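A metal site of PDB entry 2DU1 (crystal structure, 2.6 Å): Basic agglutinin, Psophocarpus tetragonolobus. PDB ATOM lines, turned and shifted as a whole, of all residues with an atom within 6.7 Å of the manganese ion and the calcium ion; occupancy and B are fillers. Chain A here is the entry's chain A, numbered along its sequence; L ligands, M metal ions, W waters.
The backbone NH (N) of Gly 105 lies within hydrogen-bond range of an oxygen (O5) of the ligand, at 2.9 Å.
The side-chain amide nitrogen of Asn 128 sits at hydrogen-bond distance from an oxygen (O5) of the ligand (3.1 Å).
OD2 of Asp 87 sits at hydrogen-bond distance from O5 of the ligand.
NE of Arg 127 lies within hydrogen-bond range of O of Asp 131.
The backbone NH of Glu 122 lies within hydrogen-bond range of the backbone carbonyl oxygen of Gly 138.
OD1 of Asp 131 sits close to NE1 of Trp 130, at 3.2 Å.
Along chain A the residues within 4 Å of the manganese ion span positions 122 to 136.
Four residues have an atom within 4 Å of the calcium ion: Asp 124, Phe 126, Asn 128 and Asp 131.
The manganese ion is bound by a ring nitrogen (NE2) of His 136 (2.3 Å), water W1 (2.3 Å), the side-chain carboxylate of Glu 122 (2.3 Å), the side-chain carboxylate of Asp 124 (2.3 Å), the side-chain carboxylate of Asp 131 (2.4 Å) and water W2 (2.4 Å).
OD1 of Asp 124 binds the calcium ion.
The calcium ion is bound by water W3 (2.4 Å).
The backbone carbonyl oxygen (O) of Phe 126 is bound to the calcium ion (2.4 Å).
The side-chain carboxylate (OD2) of Asp 131 binds the calcium ion, at 2.5 Å.
The side-chain amide oxygen (OD1) of Asn 128 is bound to the calcium ion (2.5 Å).
OD2 of Asp 124 binds the calcium ion, at 2.6 Å.
The calcium ion has six donor atoms within binding distance.
Water W1 lies within hydrogen-bond range of the backbone carbonyl oxygen (O) of Val 144 (2.8 Å), the side-chain carboxylate (OE1) of Glu 122 (2.9 Å) and the indole nitrogen (NE1) of Trp 130 (3.3 Å).
Water W3 bridges the backbone carbonyl oxygen (O) of Gly 105 (2.8 Å) and the indole nitrogen (NE1) of Trp 130 (3.3 Å).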
ATOM      1  N   ASP A  87       3.756  13.352   1.098  1.00  0.00           N
ATOM      2  CA  ASP A  87       2.540  13.690   0.370  1.00  0.00           C
ATOM      3  C   ASP A  87       2.676  15.004  -0.399  1.00  0.00           C
ATOM      4  O   ASP A  87       1.952  15.250  -1.372  1.00  0.00           O
ATOM      5  CB  ASP A  87       1.356  13.788   1.342  1.00  0.00           C
ATOM      6  CG  ASP A  87       0.665  12.462   1.545  1.00  0.00           C
ATOM      7  OD1 ASP A  87       1.122  11.684   2.428  1.00  0.00           O
ATOM      8  OD2 ASP A  87      -0.322  12.185   0.828  1.00  0.00           O
ATOM      9  N   GLY A 104      -1.166  13.147   5.941  1.00  0.00           N
ATOM     10  CA  GLY A 104      -1.438  12.544   4.641  1.00  0.00           C
ATOM     11  C   GLY A 104      -1.828  13.554   3.572  1.00  0.00           C
ATOM     12  O   GLY A 104      -1.260  14.651   3.509  1.00  0.00           O
ATOM     13  N   GLY A 105      -2.788  13.183   2.735  1.00  0.00           N
ATOM     14  CA  GLY A 105      -3.232  14.048   1.668  1.00  0.00           C
ATOM     15  C   GLY A 105      -3.814  15.371   2.096  1.00  0.00           C
ATOM     16  O   GLY A 105      -4.110  16.205   1.246  1.00  0.00           O
ATOM     17  N   TYR A 106      -3.974  15.577   3.402  1.00  0.00           N
ATOM     18  CA  TYR A 106      -4.519  16.857   3.889  1.00  0.00           C
ATOM     19  C   TYR A 106      -3.423  17.838   4.274  1.00  0.00           C
ATOM     20  O   TYR A 106      -3.697  18.953   4.701  1.00  0.00           O
ATOM     21  CB  TYR A 106      -5.466  16.630   5.062  1.00  0.00           C
ATOM     22  CG  TYR A 106      -6.702  15.853   4.680  1.00  0.00           C
ATOM     23  CD1 TYR A 106      -7.652  16.387   3.817  1.00  0.00           C
ATOM     24  CD2 TYR A 106      -6.889  14.558   5.150  1.00  0.00           C
ATOM     25  CE1 TYR A 106      -8.760  15.636   3.411  1.00  0.00           C
ATOM     26  CE2 TYR A 106      -7.997  13.804   4.758  1.00  0.00           C
ATOM     27  CZ  TYR A 106      -8.929  14.350   3.891  1.00  0.00           C
ATOM     28  OH  TYR A 106     -10.015  13.586   3.495  1.00  0.00           O
ATOM     29  N   PHE A 107      -2.176  17.403   4.119  1.00  0.00           N
ATOM     30  CA  PHE A 107      -1.017  18.260   4.358  1.00  0.00           C
ATOM     31  C   PHE A 107      -0.895  18.851   5.752  1.00  0.00           C
ATOM     32  O   PHE A 107       0.041  19.605   6.023  1.00  0.00           O
ATOM     33  CB  PHE A 107      -1.030  19.406   3.343  1.00  0.00           C
ATOM     34  CG  PHE A 107      -1.217  18.969   1.912  1.00  0.00           C
ATOM     35  CD1 PHE A 107      -0.215  18.277   1.239  1.00  0.00           C
ATOM     36  CD2 PHE A 107      -2.386  19.278   1.218  1.00  0.00           C
ATOM     37  CE1 PHE A 107      -0.364  17.903  -0.119  1.00  0.00           C
ATOM     38  CE2 PHE A 107      -2.545  18.920  -0.135  1.00  0.00           C
ATOM     39  CZ  PHE A 107      -1.542  18.238  -0.799  1.00  0.00           C
ATOM     40  N   GLU A 122      -0.611  24.300  -3.257  1.00  0.00           N
ATOM     41  CA  GLU A 122      -0.003  23.010  -2.997  1.00  0.00           C
ATOM     42  C   GLU A 122       0.936  22.497  -4.081  1.00  0.00           C
ATOM     43  O   GLU A 122       0.804  22.836  -5.259  1.00  0.00           O
ATOM     44  CB  GLU A 122      -1.092  21.945  -2.797  1.00  0.00           C
ATOM     45  CG  GLU A 122      -1.847  21.631  -4.087  1.00  0.00           C
ATOM     46  CD  GLU A 122      -2.869  20.503  -3.944  1.00  0.00           C
ATOM     47  OE1 GLU A 122      -3.692  20.559  -3.006  1.00  0.00           O
ATOM     48  OE2 GLU A 122      -2.860  19.588  -4.785  1.00  0.00           O
ATOM     49  N   ASP A 124       1.589  18.948  -4.702  1.00  0.00           N
ATOM     50  CA  ASP A 124       1.113  17.610  -4.414  1.00  0.00           C
ATOM     51  C   ASP A 124       1.931  16.538  -5.100  1.00  0.00           C
ATOM     52  O   ASP A 124       2.062  16.546  -6.327  1.00  0.00           O
ATOM     53  CB  ASP A 124      -0.338  17.518  -4.893  1.00  0.00           C
ATOM     54  CG  ASP A 124      -1.135  16.462  -4.139  1.00  0.00           C
ATOM     55  OD1 ASP A 124      -0.630  15.348  -3.915  1.00  0.00           O
ATOM     56  OD2 ASP A 124      -2.286  16.765  -3.789  1.00  0.00           O
ATOM     57  N   THR A 125       2.453  15.588  -4.323  1.00  0.00           N
ATOM     58  CA  THR A 125       3.276  14.516  -4.877  1.00  0.00           C
ATOM     59  C   THR A 125       2.620  13.128  -4.839  1.00  0.00           C
ATOM     60  O   THR A 125       3.110  12.190  -5.447  1.00  0.00           O
ATOM     61  CB  THR A 125       4.651  14.466  -4.160  1.00  0.00           C
ATOM     62  OG1 THR A 125       4.482  14.435  -2.731  1.00  0.00           O
ATOM     63  CG2 THR A 125       5.479  15.690  -4.551  1.00  0.00           C
ATOM     64  N   PHE A 126       1.492  13.010  -4.131  1.00  0.00           N
ATOM     65  CA  PHE A 126       0.777  11.740  -4.044  1.00  0.00           C
ATOM     66  C   PHE A 126      -0.627  11.882  -4.597  1.00  0.00           C
ATOM     67  O   PHE A 126      -1.346  12.829  -4.265  1.00  0.00           O
ATOM     68  CB  PHE A 126       0.670  11.289  -2.588  1.00  0.00           C
ATOM     69  CG  PHE A 126      -0.052   9.994  -2.434  1.00  0.00           C
ATOM     70  CD1 PHE A 126       0.619   8.789  -2.617  1.00  0.00           C
ATOM     71  CD2 PHE A 126      -1.417   9.975  -2.153  1.00  0.00           C
ATOM     72  CE1 PHE A 126      -0.069   7.567  -2.512  1.00  0.00           C
ATOM     73  CE2 PHE A 126      -2.110   8.775  -2.049  1.00  0.00           C
ATOM     74  CZ  PHE A 126      -1.439   7.570  -2.233  1.00  0.00           C
ATOM     75  N   ARG A 127      -1.036  10.927  -5.415  1.00  0.00           N
ATOM     76  CA  ARG A 127      -2.367  10.982  -6.010  1.00  0.00           C
ATOM     77  C   ARG A 127      -3.462  10.376  -5.150  1.00  0.00           C
ATOM     78  O   ARG A 127      -3.595   9.160  -5.073  1.00  0.00           O
ATOM     79  CB  ARG A 127      -2.364  10.305  -7.382  1.00  0.00           C
ATOM     80  CG  ARG A 127      -3.676  10.502  -8.125  1.00  0.00           C
ATOM     81  CD  ARG A 127      -3.596  10.107  -9.584  1.00  0.00           C
ATOM     82  NE  ARG A 127      -4.773  10.610 -10.293  1.00  0.00           N
ATOM     83  CZ  ARG A 127      -5.048  10.365 -11.574  1.00  0.00           C
ATOM     84  NH1 ARG A 127      -4.233   9.606 -12.296  1.00  0.00           N
ATOM     85  NH2 ARG A 127      -6.142  10.887 -12.130  1.00  0.00           N
ATOM     86  N   ASN A 128      -4.261  11.230  -4.507  1.00  0.00           N
ATOM     87  CA  ASN A 128      -5.382  10.758  -3.700  1.00  0.00           C
ATOM     88  C   ASN A 128      -6.556  10.563  -4.640  1.00  0.00           C
ATOM     89  O   ASN A 128      -6.478  10.911  -5.813  1.00  0.00           O
ATOM     90  CB  ASN A 128      -5.737  11.783  -2.611  1.00  0.00           C
ATOM     91  CG  ASN A 128      -4.734  11.862  -1.478  1.00  0.00           C
ATOM     92  OD1 ASN A 128      -3.797  12.664  -1.530  1.00  0.00           O
ATOM     93  ND2 ASN A 128      -4.923  11.048  -0.453  1.00  0.00           N
ATOM     94  N   TRP A 130      -9.127  12.169  -5.006  1.00  0.00           N
ATOM     95  CA  TRP A 130      -9.595  13.445  -5.535  1.00  0.00           C
ATOM     96  C   TRP A 130      -8.559  14.199  -6.366  1.00  0.00           C
ATOM     97  O   TRP A 130      -8.804  15.335  -6.769  1.00  0.00           O
ATOM     98  CB  TRP A 130     -10.032  14.337  -4.378  1.00  0.00           C
ATOM     99  CG  TRP A 130      -8.907  14.626  -3.448  1.00  0.00           C
ATOM    100  CD1 TRP A 130      -7.839  15.446  -3.688  1.00  0.00           C
ATOM    101  CD2 TRP A 130      -8.675  14.037  -2.159  1.00  0.00           C
ATOM    102  NE1 TRP A 130      -6.958  15.409  -2.635  1.00  0.00           N
ATOM    103  CE2 TRP A 130      -7.451  14.547  -1.683  1.00  0.00           C
ATOM    104  CE3 TRP A 130      -9.391  13.129  -1.365  1.00  0.00           C
ATOM    105  CZ2 TRP A 130      -6.915  14.187  -0.435  1.00  0.00           C
ATOM    106  CZ3 TRP A 130      -8.861  12.767  -0.124  1.00  0.00           C
ATOM    107  CH2 TRP A 130      -7.644  13.292   0.327  1.00  0.00           C
ATOM    108  N   ASP A 131      -7.406  13.564  -6.618  1.00  0.00           N
ATOM    109  CA  ASP A 131      -6.319  14.183  -7.378  1.00  0.00           C
ATOM    110  C   ASP A 131      -6.151  13.764  -8.813  1.00  0.00           C
ATOM    111  O   ASP A 131      -6.489  12.637  -9.189  1.00  0.00           O
ATOM    112  CB  ASP A 131      -4.940  13.893  -6.751  1.00  0.00           C
ATOM    113  CG  ASP A 131      -4.750  14.664  -5.491  1.00  0.00           C
ATOM    114  OD1 ASP A 131      -5.343  15.763  -5.362  1.00  0.00           O
ATOM    115  OD2 ASP A 131      -3.960  14.191  -4.640  1.00  0.00           O
ATOM    116  N   PRO A 132      -5.612  14.667  -9.640  1.00  0.00           N
ATOM    117  CA  PRO A 132      -5.354  14.383 -11.053  1.00  0.00           C
ATOM    118  C   PRO A 132      -3.928  13.837 -10.985  1.00  0.00           C
ATOM    119  O   PRO A 132      -3.386  13.684  -9.889  1.00  0.00           O
ATOM    120  CB  PRO A 132      -5.442  15.762 -11.696  1.00  0.00           C
ATOM    121  CG  PRO A 132      -4.959  16.667 -10.633  1.00  0.00           C
ATOM    122  CD  PRO A 132      -5.651  16.119  -9.398  1.00  0.00           C
ATOM    123  N   ILE A 134       0.006  13.275 -10.659  1.00  0.00           N
ATOM    124  CA  ILE A 134       0.971  13.998  -9.849  1.00  0.00           C
ATOM    125  C   ILE A 134       2.352  13.868 -10.498  1.00  0.00           C
ATOM    126  O   ILE A 134       2.566  12.994 -11.328  1.00  0.00           O
ATOM    127  CB  ILE A 134       1.027  13.455  -8.390  1.00  0.00           C
ATOM    128  CG1 ILE A 134       1.192  11.932  -8.373  1.00  0.00           C
ATOM    129  CG2 ILE A 134      -0.222  13.859  -7.643  1.00  0.00           C
ATOM    130  CD1 ILE A 134       2.620  11.435  -8.549  1.00  0.00           C
ATOM    131  N   HIS A 136       1.678  17.854  -9.091  1.00  0.00           N
ATOM    132  CA  HIS A 136       0.950  18.975  -9.649  1.00  0.00           C
ATOM    133  C   HIS A 136       0.877  20.128  -8.677  1.00  0.00           C
ATOM    134  O   HIS A 136       1.039  19.968  -7.463  1.00  0.00           O
ATOM    135  CB  HIS A 136      -0.463  18.568 -10.094  1.00  0.00           C
ATOM    136  CG  HIS A 136      -1.326  17.972  -9.020  1.00  0.00           C
ATOM    137  ND1 HIS A 136      -1.588  16.626  -8.945  1.00  0.00           N
ATOM    138  CD2 HIS A 136      -1.981  18.543  -7.983  1.00  0.00           C
ATOM    139  CE1 HIS A 136      -2.379  16.382  -7.918  1.00  0.00           C
ATOM    140  NE2 HIS A 136      -2.631  17.532  -7.315  1.00  0.00           N
ATOM    141  N   ILE A 137       0.664  21.316  -9.229  1.00  0.00           N
ATOM    142  CA  ILE A 137       0.505  22.530  -8.440  1.00  0.00           C
ATOM    143  C   ILE A 137      -0.996  22.704  -8.401  1.00  0.00           C
ATOM    144  O   ILE A 137      -1.667  22.469  -9.405  1.00  0.00           O
ATOM    145  CB  ILE A 137       1.094  23.759  -9.151  1.00  0.00           C
ATOM    146  CG1 ILE A 137       2.550  23.496  -9.561  1.00  0.00           C
ATOM    147  CG2 ILE A 137       1.012  24.952  -8.248  1.00  0.00           C
ATOM    148  CD1 ILE A 137       3.124  24.583 -10.439  1.00  0.00           C
ATOM    149  N   GLY A 138      -1.513  23.101  -7.264  1.00  0.00           N
ATOM    150  CA  GLY A 138      -2.939  23.291  -7.160  1.00  0.00           C
ATOM    151  C   GLY A 138      -3.273  24.478  -6.279  1.00  0.00           C
ATOM    152  O   GLY A 138      -2.511  24.810  -5.366  1.00  0.00           O
ATOM    153  N   ASP A 140      -5.902  25.734  -3.660  1.00  0.00           N
ATOM    154  CA  ASP A 140      -6.950  25.241  -2.790  1.00  0.00           C
ATOM    155  C   ASP A 140      -7.618  26.315  -1.953  1.00  0.00           C
ATOM    156  O   ASP A 140      -6.964  27.141  -1.330  1.00  0.00           O
ATOM    157  CB  ASP A 140      -6.379  24.160  -1.875  1.00  0.00           C
ATOM    158  CG  ASP A 140      -5.613  23.076  -2.633  1.00  0.00           C
ATOM    159  OD1 ASP A 140      -5.927  22.842  -3.828  1.00  0.00           O
ATOM    160  OD2 ASP A 140      -4.706  22.460  -2.037  1.00  0.00           O
ATOM    161  N   VAL A 144      -8.866  20.591  -0.075  1.00  0.00           N
ATOM    162  CA  VAL A 144      -7.679  20.097  -0.731  1.00  0.00           C
ATOM    163  C   VAL A 144      -8.074  19.616  -2.131  1.00  0.00           C
ATOM    164  O   VAL A 144      -7.292  18.992  -2.845  1.00  0.00           O
ATOM    165  CB  VAL A 144      -7.060  18.951   0.091  1.00  0.00           C
ATOM    166  CG1 VAL A 144      -8.034  17.791   0.201  1.00  0.00           C
ATOM    167  CG2 VAL A 144      -5.755  18.528  -0.511  1.00  0.00           C
ATOM    168  N   ILE A 145      -9.323  19.900  -2.504  1.00  0.00           N
ATOM    169  CA  ILE A 145      -9.822  19.553  -3.833  1.00  0.00           C
ATOM    170  C   ILE A 145      -9.638  20.834  -4.636  1.00  0.00           C
ATOM    171  O   ILE A 145     -10.542  21.657  -4.733  1.00  0.00           O
ATOM    172  CB  ILE A 145     -11.295  19.173  -3.798  1.00  0.00           C
ATOM    173  CG1 ILE A 145     -11.475  17.908  -2.962  1.00  0.00           C
ATOM    174  CG2 ILE A 145     -11.809  18.959  -5.202  1.00  0.00           C
ATOM    175  CD1 ILE A 145     -12.893  17.384  -2.939  1.00  0.00           C
ATOM    176  N   SER A 146      -8.436  20.997  -5.176  1.00  0.00           N
ATOM    177  CA  SER A 146      -8.045  22.189  -5.935  1.00  0.00           C
ATOM    178  C   SER A 146      -9.063  22.718  -6.926  1.00  0.00           C
ATOM    179  O   SER A 146      -9.763  21.961  -7.594  1.00  0.00           O
ATOM    180  CB  SER A 146      -6.744  21.906  -6.691  1.00  0.00           C
ATOM    181  OG  SER A 146      -5.735  21.475  -5.799  1.00  0.00           O
ATOM    182  N   THR A 149      -5.515  23.157 -11.248  1.00  0.00           N
ATOM    183  CA  THR A 149      -4.351  22.299 -11.140  1.00  0.00           C
ATOM    184  C   THR A 149      -3.485  22.332 -12.409  1.00  0.00           C
ATOM    185  O   THR A 149      -3.995  22.543 -13.507  1.00  0.00           O
ATOM    186  CB  THR A 149      -4.850  20.829 -10.906  1.00  0.00           C
ATOM    187  OG1 THR A 149      -4.878  20.543  -9.508  1.00  0.00           O
ATOM    188  CG2 THR A 149      -3.997  19.830 -11.641  1.00  0.00           C
HETATM  189  O1  LIG L   1       0.649   5.270   1.541  1.00  0.00           O
HETATM  190  C1  LIG L   1       0.628   6.694   1.505  1.00  0.00           C
HETATM  191  C2  LIG L   1      -0.795   7.221   1.425  1.00  0.00           C
HETATM  192  O2  LIG L   1      -1.542   6.735   2.584  1.00  0.00           O
HETATM  193  C3  LIG L   1      -2.968   7.157   2.602  1.00  0.00           C
HETATM  194  O3  LIG L   1      -3.775   6.608   1.541  1.00  0.00           O
HETATM  195  C4  LIG L   1      -3.837   5.182   1.407  1.00  0.00           C
HETATM  196  C5  LIG L   1      -3.040   8.704   2.578  1.00  0.00           C
HETATM  197  N1  LIG L   1      -4.445   9.122   2.578  1.00  0.00           N
HETATM  198  C6  LIG L   1      -4.905  10.058   3.417  1.00  0.00           C
HETATM  199  O4  LIG L   1      -4.212  10.653   4.242  1.00  0.00           O
HETATM  200  C7  LIG L   1      -6.393  10.398   3.294  1.00  0.00           C
HETATM  201  C8  LIG L   1      -2.298   9.239   1.329  1.00  0.00           C
HETATM  202  O5  LIG L   1      -2.366  10.661   1.280  1.00  0.00           O
HETATM  203  C9  LIG L   1      -0.828   8.775   1.378  1.00  0.00           C
HETATM  204  O6  LIG L   1      -0.175   9.333   2.532  1.00  0.00           O
HETATM  205 MN    MN M   1      -3.822  17.564  -5.358  1.00  0.00          MN
HETATM  206 CA    CA M   2      -2.403  14.404  -2.740  1.00  0.00          CA
HETATM  207  O   HOH W   1      -4.775  17.868  -3.273  1.00  0.00           O
HETATM  208  O   HOH W   2      -5.638  18.880  -6.096  1.00  0.00           O
HETATM  209  O   HOH W   3      -3.926  15.787  -1.477  1.00  0.00           O
